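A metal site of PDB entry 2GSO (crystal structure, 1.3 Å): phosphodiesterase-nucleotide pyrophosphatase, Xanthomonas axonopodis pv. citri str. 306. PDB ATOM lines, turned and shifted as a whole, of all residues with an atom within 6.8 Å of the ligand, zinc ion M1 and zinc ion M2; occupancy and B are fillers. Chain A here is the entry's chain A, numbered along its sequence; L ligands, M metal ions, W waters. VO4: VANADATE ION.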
ATOM      1  N   ILE A  14       3.385   3.986 -22.375  1.00  0.00           N
ATOM      2  CA  ILE A  14       2.526   3.695 -21.247  1.00  0.00           C
ATOM      3  C   ILE A  14       3.032   4.610 -20.116  1.00  0.00           C
ATOM      4  O   ILE A  14       4.031   4.310 -19.439  1.00  0.00           O
ATOM      5  CB  ILE A  14       2.560   2.209 -20.848  1.00  0.00           C
ATOM      6  CG1 ILE A  14       2.218   1.335 -22.064  1.00  0.00           C
ATOM      7  CG2 ILE A  14       1.588   1.977 -19.695  1.00  0.00           C
ATOM      8  CD1 ILE A  14       2.421  -0.140 -21.848  1.00  0.00           C
ATOM      9  N   ASP A  15       2.373   5.744 -19.937  1.00  0.00           N
ATOM     10  CA  ASP A  15       2.815   6.742 -18.981  1.00  0.00           C
ATOM     11  C   ASP A  15       2.966   6.133 -17.585  1.00  0.00           C
ATOM     12  O   ASP A  15       2.060   5.445 -17.103  1.00  0.00           O
ATOM     13  CB  ASP A  15       1.819   7.919 -18.994  1.00  0.00           C
ATOM     14  CG  ASP A  15       2.390   9.180 -18.416  1.00  0.00           C
ATOM     15  OD1 ASP A  15       3.133   9.062 -17.438  1.00  0.00           O
ATOM     16  OD2 ASP A  15       2.163  10.265 -18.993  1.00  0.00           O
ATOM     17  N   GLY A  16       4.114   6.316 -16.938  1.00  0.00           N
ATOM     18  CA  GLY A  16       4.292   5.922 -15.547  1.00  0.00           C
ATOM     19  C   GLY A  16       4.428   4.448 -15.244  1.00  0.00           C
ATOM     20  O   GLY A  16       4.290   4.054 -14.096  1.00  0.00           O
ATOM     21  N   SER A  49      12.380  13.775 -14.012  1.00  0.00           N
ATOM     22  CA  SER A  49      11.631  12.546 -14.360  1.00  0.00           C
ATOM     23  C   SER A  49      10.127  12.794 -14.443  1.00  0.00           C
ATOM     24  O   SER A  49       9.329  12.157 -13.726  1.00  0.00           O
ATOM     25  CB  SER A  49      11.946  11.405 -13.381  1.00  0.00           C
ATOM     26  OG  SER A  49      11.749  11.818 -12.047  1.00  0.00           O
ATOM     27  N   LEU A  50       9.758  13.712 -15.321  1.00  0.00           N
ATOM     28  CA  LEU A  50       8.399  14.177 -15.501  1.00  0.00           C
ATOM     29  C   LEU A  50       7.935  13.878 -16.936  1.00  0.00           C
ATOM     30  O   LEU A  50       8.749  13.601 -17.828  1.00  0.00           O
ATOM     31  CB  LEU A  50       8.302  15.685 -15.206  1.00  0.00           C
ATOM     32  CG  LEU A  50       8.639  16.110 -13.774  1.00  0.00           C
ATOM     33  CD1 LEU A  50       8.656  17.613 -13.672  1.00  0.00           C
ATOM     34  CD2 LEU A  50       7.651  15.511 -12.801  1.00  0.00           C
ATOM     35  N   THR A  51       6.627  13.961 -17.166  1.00  0.00           N
ATOM     36  CA  THR A  51       6.023  13.502 -18.419  1.00  0.00           C
ATOM     37  C   THR A  51       6.411  14.248 -19.664  1.00  0.00           C
ATOM     38  O   THR A  51       6.805  13.626 -20.644  1.00  0.00           O
ATOM     39  CB  THR A  51       4.508  13.576 -18.293  1.00  0.00           C
ATOM     40  OG1 THR A  51       4.112  12.700 -17.259  1.00  0.00           O
ATOM     41  CG2 THR A  51       3.790  13.137 -19.569  1.00  0.00           C
ATOM     42  N   PHE A  52       6.253  15.558 -19.682  1.00  0.00           N
ATOM     43  CA  PHE A  52       6.498  16.290 -20.911  1.00  0.00           C
ATOM     44  C   PHE A  52       7.984  16.275 -21.270  1.00  0.00           C
ATOM     45  O   PHE A  52       8.341  15.942 -22.409  1.00  0.00           O
ATOM     46  CB  PHE A  52       5.878  17.702 -20.890  1.00  0.00           C
ATOM     47  CG  PHE A  52       4.539  17.777 -21.580  1.00  0.00           C
ATOM     48  CD1 PHE A  52       3.552  16.825 -21.347  1.00  0.00           C
ATOM     49  CD2 PHE A  52       4.266  18.804 -22.474  1.00  0.00           C
ATOM     50  CE1 PHE A  52       2.313  16.886 -21.988  1.00  0.00           C
ATOM     51  CE2 PHE A  52       3.022  18.870 -23.130  1.00  0.00           C
ATOM     52  CZ  PHE A  52       2.061  17.909 -22.884  1.00  0.00           C
ATOM     53  N   PRO A  53       8.863  16.588 -20.301  1.00  0.00           N
ATOM     54  CA  PRO A  53      10.278  16.503 -20.592  1.00  0.00           C
ATOM     55  C   PRO A  53      10.719  15.156 -21.172  1.00  0.00           C
ATOM     56  O   PRO A  53      11.462  15.107 -22.133  1.00  0.00           O
ATOM     57  CB  PRO A  53      10.924  16.797 -19.235  1.00  0.00           C
ATOM     58  CG  PRO A  53       9.943  17.694 -18.560  1.00  0.00           C
ATOM     59  CD  PRO A  53       8.612  17.132 -18.957  1.00  0.00           C
ATOM     60  N   HIS A  55       8.806  12.505 -22.498  1.00  0.00           N
ATOM     61  CA  HIS A  55       8.221  12.127 -23.772  1.00  0.00           C
ATOM     62  C   HIS A  55       8.941  12.873 -24.900  1.00  0.00           C
ATOM     63  O   HIS A  55       9.169  12.298 -25.967  1.00  0.00           O
ATOM     64  CB  HIS A  55       6.722  12.421 -23.856  1.00  0.00           C
ATOM     65  CG  HIS A  55       5.855  11.355 -23.261  1.00  0.00           C
ATOM     66  ND1 HIS A  55       5.517  11.341 -21.935  1.00  0.00           N
ATOM     67  CD2 HIS A  55       5.266  10.251 -23.808  1.00  0.00           C
ATOM     68  CE1 HIS A  55       4.750  10.289 -21.682  1.00  0.00           C
ATOM     69  NE2 HIS A  55       4.591   9.611 -22.799  1.00  0.00           N
ATOM     70  N   ASN A  72       7.126  20.290 -16.749  1.00  0.00           N
ATOM     71  CA  ASN A  72       5.750  20.357 -17.244  1.00  0.00           C
ATOM     72  C   ASN A  72       5.185  21.792 -17.191  1.00  0.00           C
ATOM     73  O   ASN A  72       4.322  22.133 -17.987  1.00  0.00           O
ATOM     74  CB  ASN A  72       4.828  19.472 -16.395  1.00  0.00           C
ATOM     75  CG  ASN A  72       5.066  17.979 -16.583  1.00  0.00           C
ATOM     76  OD1 ASN A  72       5.511  17.512 -17.633  1.00  0.00           O
ATOM     77  ND2 ASN A  72       4.723  17.205 -15.558  1.00  0.00           N
ATOM     78  N   LEU A  84       0.446  22.127 -18.893  1.00  0.00           N
ATOM     79  CA  LEU A  84      -0.122  21.081 -19.741  1.00  0.00           C
ATOM     80  C   LEU A  84      -1.513  21.424 -20.268  1.00  0.00           C
ATOM     81  O   LEU A  84      -1.876  20.990 -21.358  1.00  0.00           O
ATOM     82  CB  LEU A  84      -0.106  19.724 -19.027  1.00  0.00           C
ATOM     83  CG  LEU A  84       1.259  19.241 -18.505  1.00  0.00           C
ATOM     84  CD1 LEU A  84       1.246  17.747 -18.180  1.00  0.00           C
ATOM     85  CD2 LEU A  84       2.387  19.551 -19.501  1.00  0.00           C
ATOM     86  N   TYR A 166      -0.492   6.521 -27.018  1.00  0.00           N
ATOM     87  CA  TYR A 166      -0.184   6.985 -25.666  1.00  0.00           C
ATOM     88  C   TYR A 166      -1.289   6.533 -24.731  1.00  0.00           C
ATOM     89  O   TYR A 166      -2.472   6.632 -25.095  1.00  0.00           O
ATOM     90  CB  TYR A 166      -0.061   8.502 -25.623  1.00  0.00           C
ATOM     91  CG  TYR A 166      -0.036   9.084 -24.233  1.00  0.00           C
ATOM     92  CD1 TYR A 166       1.129   9.135 -23.489  1.00  0.00           C
ATOM     93  CD2 TYR A 166      -1.207   9.563 -23.639  1.00  0.00           C
ATOM     94  CE1 TYR A 166       1.147   9.662 -22.213  1.00  0.00           C
ATOM     95  CE2 TYR A 166      -1.204  10.084 -22.365  1.00  0.00           C
ATOM     96  CZ  TYR A 166      -0.033  10.116 -21.649  1.00  0.00           C
ATOM     97  OH  TYR A 166      -0.023  10.649 -20.374  1.00  0.00           O
ATOM     98  N   ASP A 171      -0.282   5.858 -15.088  1.00  0.00           N
ATOM     99  CA  ASP A 171       0.196   7.024 -14.357  1.00  0.00           C
ATOM    100  C   ASP A 171      -0.884   7.565 -13.424  1.00  0.00           C
ATOM    101  O   ASP A 171      -0.625   7.858 -12.260  1.00  0.00           O
ATOM    102  CB  ASP A 171       0.671   8.112 -15.328  1.00  0.00           C
ATOM    103  CG  ASP A 171       1.211   9.316 -14.609  1.00  0.00           C
ATOM    104  OD1 ASP A 171       2.312   9.184 -14.028  1.00  0.00           O
ATOM    105  OD2 ASP A 171       0.573  10.390 -14.682  1.00  0.00           O
ATOM    106  N   GLU A 172      -2.105   7.723 -13.936  1.00  0.00           N
ATOM    107  CA  GLU A 172      -3.199   8.282 -13.151  1.00  0.00           C
ATOM    108  C   GLU A 172      -3.513   7.436 -11.922  1.00  0.00           C
ATOM    109  O   GLU A 172      -3.672   7.975 -10.833  1.00  0.00           O
ATOM    110  CB  GLU A 172      -4.440   8.485 -14.023  1.00  0.00           C
ATOM    111  CG  GLU A 172      -4.237   9.531 -15.118  1.00  0.00           C
ATOM    112  CD  GLU A 172      -5.529   9.967 -15.824  1.00  0.00           C
ATOM    113  OE1 GLU A 172      -6.622   9.443 -15.497  1.00  0.00           O
ATOM    114  OE2 GLU A 172      -5.445  10.838 -16.718  1.00  0.00           O
ATOM    115  N   HIS A 175      -0.627   7.885  -9.331  1.00  0.00           N
ATOM    116  CA  HIS A 175      -0.752   9.093  -8.521  1.00  0.00           C
ATOM    117  C   HIS A 175      -1.824   8.960  -7.451  1.00  0.00           C
ATOM    118  O   HIS A 175      -1.625   9.346  -6.297  1.00  0.00           O
ATOM    119  CB  HIS A 175      -1.057  10.319  -9.373  1.00  0.00           C
ATOM    120  CG  HIS A 175       0.090  10.780 -10.206  1.00  0.00           C
ATOM    121  ND1 HIS A 175       1.213  11.365  -9.672  1.00  0.00           N
ATOM    122  CD2 HIS A 175       0.282  10.742 -11.552  1.00  0.00           C
ATOM    123  CE1 HIS A 175       2.051  11.675 -10.660  1.00  0.00           C
ATOM    124  NE2 HIS A 175       1.503  11.307 -11.806  1.00  0.00           N
ATOM    125  N   ASP A 218       7.735   6.818 -19.870  1.00  0.00           N
ATOM    126  CA  ASP A 218       8.475   8.061 -19.655  1.00  0.00           C
ATOM    127  C   ASP A 218       9.246   8.076 -18.339  1.00  0.00           C
ATOM    128  O   ASP A 218      10.270   8.727 -18.239  1.00  0.00           O
ATOM    129  CB  ASP A 218       7.539   9.268 -19.794  1.00  0.00           C
ATOM    130  CG  ASP A 218       6.301   9.191 -18.941  1.00  0.00           C
ATOM    131  OD1 ASP A 218       5.925   8.123 -18.399  1.00  0.00           O
ATOM    132  OD2 ASP A 218       5.722  10.288 -18.794  1.00  0.00           O
ATOM    133  N   HIS A 219       8.735   7.340 -17.364  1.00  0.00           N
ATOM    134  CA  HIS A 219       9.317   7.253 -16.023  1.00  0.00           C
ATOM    135  C   HIS A 219       8.531   6.215 -15.233  1.00  0.00           C
ATOM    136  O   HIS A 219       7.468   5.760 -15.683  1.00  0.00           O
ATOM    137  CB  HIS A 219       9.152   8.581 -15.293  1.00  0.00           C
ATOM    138  CG  HIS A 219       7.757   9.092 -15.352  1.00  0.00           C
ATOM    139  ND1 HIS A 219       6.730   8.516 -14.619  1.00  0.00           N
ATOM    140  CD2 HIS A 219       7.188  10.032 -16.134  1.00  0.00           C
ATOM    141  CE1 HIS A 219       5.598   9.120 -14.948  1.00  0.00           C
ATOM    142  NE2 HIS A 219       5.848  10.041 -15.854  1.00  0.00           N
ATOM    143  N   GLY A 220       9.042   5.851 -14.066  1.00  0.00           N
ATOM    144  CA  GLY A 220       8.346   4.949 -13.149  1.00  0.00           C
ATOM    145  C   GLY A 220       7.444   5.695 -12.176  1.00  0.00           C
ATOM    146  O   GLY A 220       6.817   6.682 -12.531  1.00  0.00           O
ATOM    147  N   MET A 221       7.326   5.161 -10.967  1.00  0.00           N
ATOM    148  CA  MET A 221       6.388   5.663  -9.974  1.00  0.00           C
ATOM    149  C   MET A 221       6.817   5.202  -8.601  1.00  0.00           C
ATOM    150  O   MET A 221       7.129   4.028  -8.422  1.00  0.00           O
ATOM    151  CB  MET A 221       5.000   5.104 -10.274  1.00  0.00           C
ATOM    152  CG  MET A 221       3.886   5.645  -9.398  1.00  0.00           C
ATOM    153  SD  MET A 221       3.452   7.358  -9.737  1.00  0.00           S
ATOM    154  CE  MET A 221       2.821   7.184 -11.407  1.00  0.00           C
ATOM    155  N   GLN A 248       7.714  17.773  -7.046  1.00  0.00           N
ATOM    156  CA  GLN A 248       8.984  17.148  -6.645  1.00  0.00           C
ATOM    157  C   GLN A 248      10.223  17.909  -7.128  1.00  0.00           C
ATOM    158  O   GLN A 248      11.264  17.842  -6.476  1.00  0.00           O
ATOM    159  CB  GLN A 248       9.008  15.708  -7.167  1.00  0.00           C
ATOM    160  CG  GLN A 248       7.803  14.919  -6.697  1.00  0.00           C
ATOM    161  CD  GLN A 248       6.549  15.183  -7.510  1.00  0.00           C
ATOM    162  OE1 GLN A 248       6.612  15.436  -8.716  1.00  0.00           O
ATOM    163  NE2 GLN A 248       5.392  15.146  -6.852  1.00  0.00           N
ATOM    164  N   SER A 323       4.039   9.293  -6.756  1.00  0.00           N
ATOM    165  CA  SER A 323       4.673  10.390  -7.457  1.00  0.00           C
ATOM    166  C   SER A 323       5.904   9.901  -8.183  1.00  0.00           C
ATOM    167  O   SER A 323       6.473   8.843  -7.871  1.00  0.00           O
ATOM    168  CB  SER A 323       5.091  11.509  -6.491  1.00  0.00           C
ATOM    169  OG  SER A 323       4.005  12.188  -5.934  1.00  0.00           O
ATOM    170  N   HIS A 324       6.307  10.694  -9.160  1.00  0.00           N
ATOM    171  CA  HIS A 324       7.602  10.539  -9.788  1.00  0.00           C
ATOM    172  C   HIS A 324       8.260  11.893  -9.753  1.00  0.00           C
ATOM    173  O   HIS A 324       7.986  12.653  -8.821  1.00  0.00           O
ATOM    174  CB  HIS A 324       7.445   9.920 -11.175  1.00  0.00           C
ATOM    175  CG  HIS A 324       6.400  10.572 -12.009  1.00  0.00           C
ATOM    176  ND1 HIS A 324       6.709  11.542 -12.934  1.00  0.00           N
ATOM    177  CD2 HIS A 324       5.053  10.440 -12.026  1.00  0.00           C
ATOM    178  CE1 HIS A 324       5.594  11.970 -13.496  1.00  0.00           C
ATOM    179  NE2 HIS A 324       4.578  11.319 -12.960  1.00  0.00           N
ATOM    180  N   GLY A 325       9.158  12.228 -10.673  1.00  0.00           N
ATOM    181  CA  GLY A 325       9.886  13.493 -10.555  1.00  0.00           C
ATOM    182  C   GLY A 325      11.065  13.430  -9.608  1.00  0.00           C
ATOM    183  O   GLY A 325      11.639  14.457  -9.249  1.00  0.00           O
HETATM  184  V   VO4 L   1       3.127  13.413 -15.810  1.00  0.00           V
HETATM  185  O1  VO4 L   1       4.663  14.448 -15.085  1.00  0.00           O
HETATM  186  O2  VO4 L   1       1.930  14.428 -16.628  1.00  0.00           O
HETATM  187  O3  VO4 L   1       2.959  11.403 -15.627  1.00  0.00           O
HETATM  188  O4  VO4 L   1       2.334  13.451 -14.036  1.00  0.00           O
HETATM  189 ZN    ZN M   1       4.419  10.644 -17.181  1.00  0.00          ZN
HETATM  190 ZN    ZN M   2       2.561  11.323 -13.544  1.00  0.00          ZN
HETATM  191  O   HOH W   1       0.773  12.234 -17.262  1.00  0.00           O
HETATM  192  O   HOH W   2      -0.236  14.670 -13.550  1.00  0.00           O
HETATM  193  O   HOH W   3       4.159  14.660 -12.135  1.00  0.00           O
HETATM  194  O   HOH W   4      -0.222  14.578 -18.156  1.00  0.00           O
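Zinc ion M2 is bound by a ring nitrogen (NE2) of His 175 (2.0 Å). Zinc ion M2 is bound by a ring nitrogen (NE2) of His 324 (2.1 Å). Zinc ion M2 is bound by an oxygen (O3) of the ligand (2.1 Å). O4 of the ligand binds zinc ion M2 (2.2 Å). Zinc ion M2 is bound by the side-chain carboxylate (OD1) of Asp 171, 2.2 Å away. Zinc ion M2 is bound by the side-chain carboxylate (OD2) of Asp 171 (2.5 Å). Zinc ion M2 has six donor atoms within binding distance.
An oxygen (O1) of the ligand sits close to the side-chain amide nitrogen of Asn 72 (2.8 Å). CA of Leu 50 touches O1 of the ligand, at 3.8 Å. Leu 84 touches the ligand (CD1 to O2, 3.7 Å). The nearest printed residue that does not touch the ligand is Asp 218 (4.3 Å).
Of the 23 residues printed, 3 come within 4 Å of zinc ion M2. The nearest printed residue that does not touch zinc ion M2 is His 219 (4.01 Å).
ND1 of His 219 sits close to ND1 of His 324, at 3.5 Å. The backbone carbonyl oxygen (O) of Asp 15 is in hydrogen-bond range of the backbone NH (N) of Asp 171. OD2 of Asp 15 is in hydrogen-bond range of OH of Tyr 166 (2.6 Å). The backbone carbonyl oxygen (O) of Ser 49 lies within hydrogen-bond range of a ring nitrogen (ND1) of His 324. The side-chain amide oxygen of Gln 248 sits close to the backbone carbonyl oxygen of His 324 (3.1 Å). The backbone NH of Gly 16 lies within hydrogen-bond range of the side-chain carboxylate of Asp 218 (2.9 Å). OD2 of Asp 218 lies close to ND1 of His 55 (3.3 Å). The side-chain amide oxygen (OD1) of Asn 72 is in hydrogen-bond range of the backbone NH (N) of Phe 52.
Four residues have an atom within 4 Å of zinc ion M1: Asp 15, Thr 51, Asp 218 and His 219.
Zinc ion M1 is bound by NE2 of His 219, OD1 of Asp 15, OG1 of Thr 51, OD2 of Asp 218 and O3 of the ligand. Zinc ion M1 has five donor atoms within binding distance.
The side-chain hydroxyl of Thr 51 binds a vanadium atom (V) of the ligand, 1.9 Å away.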
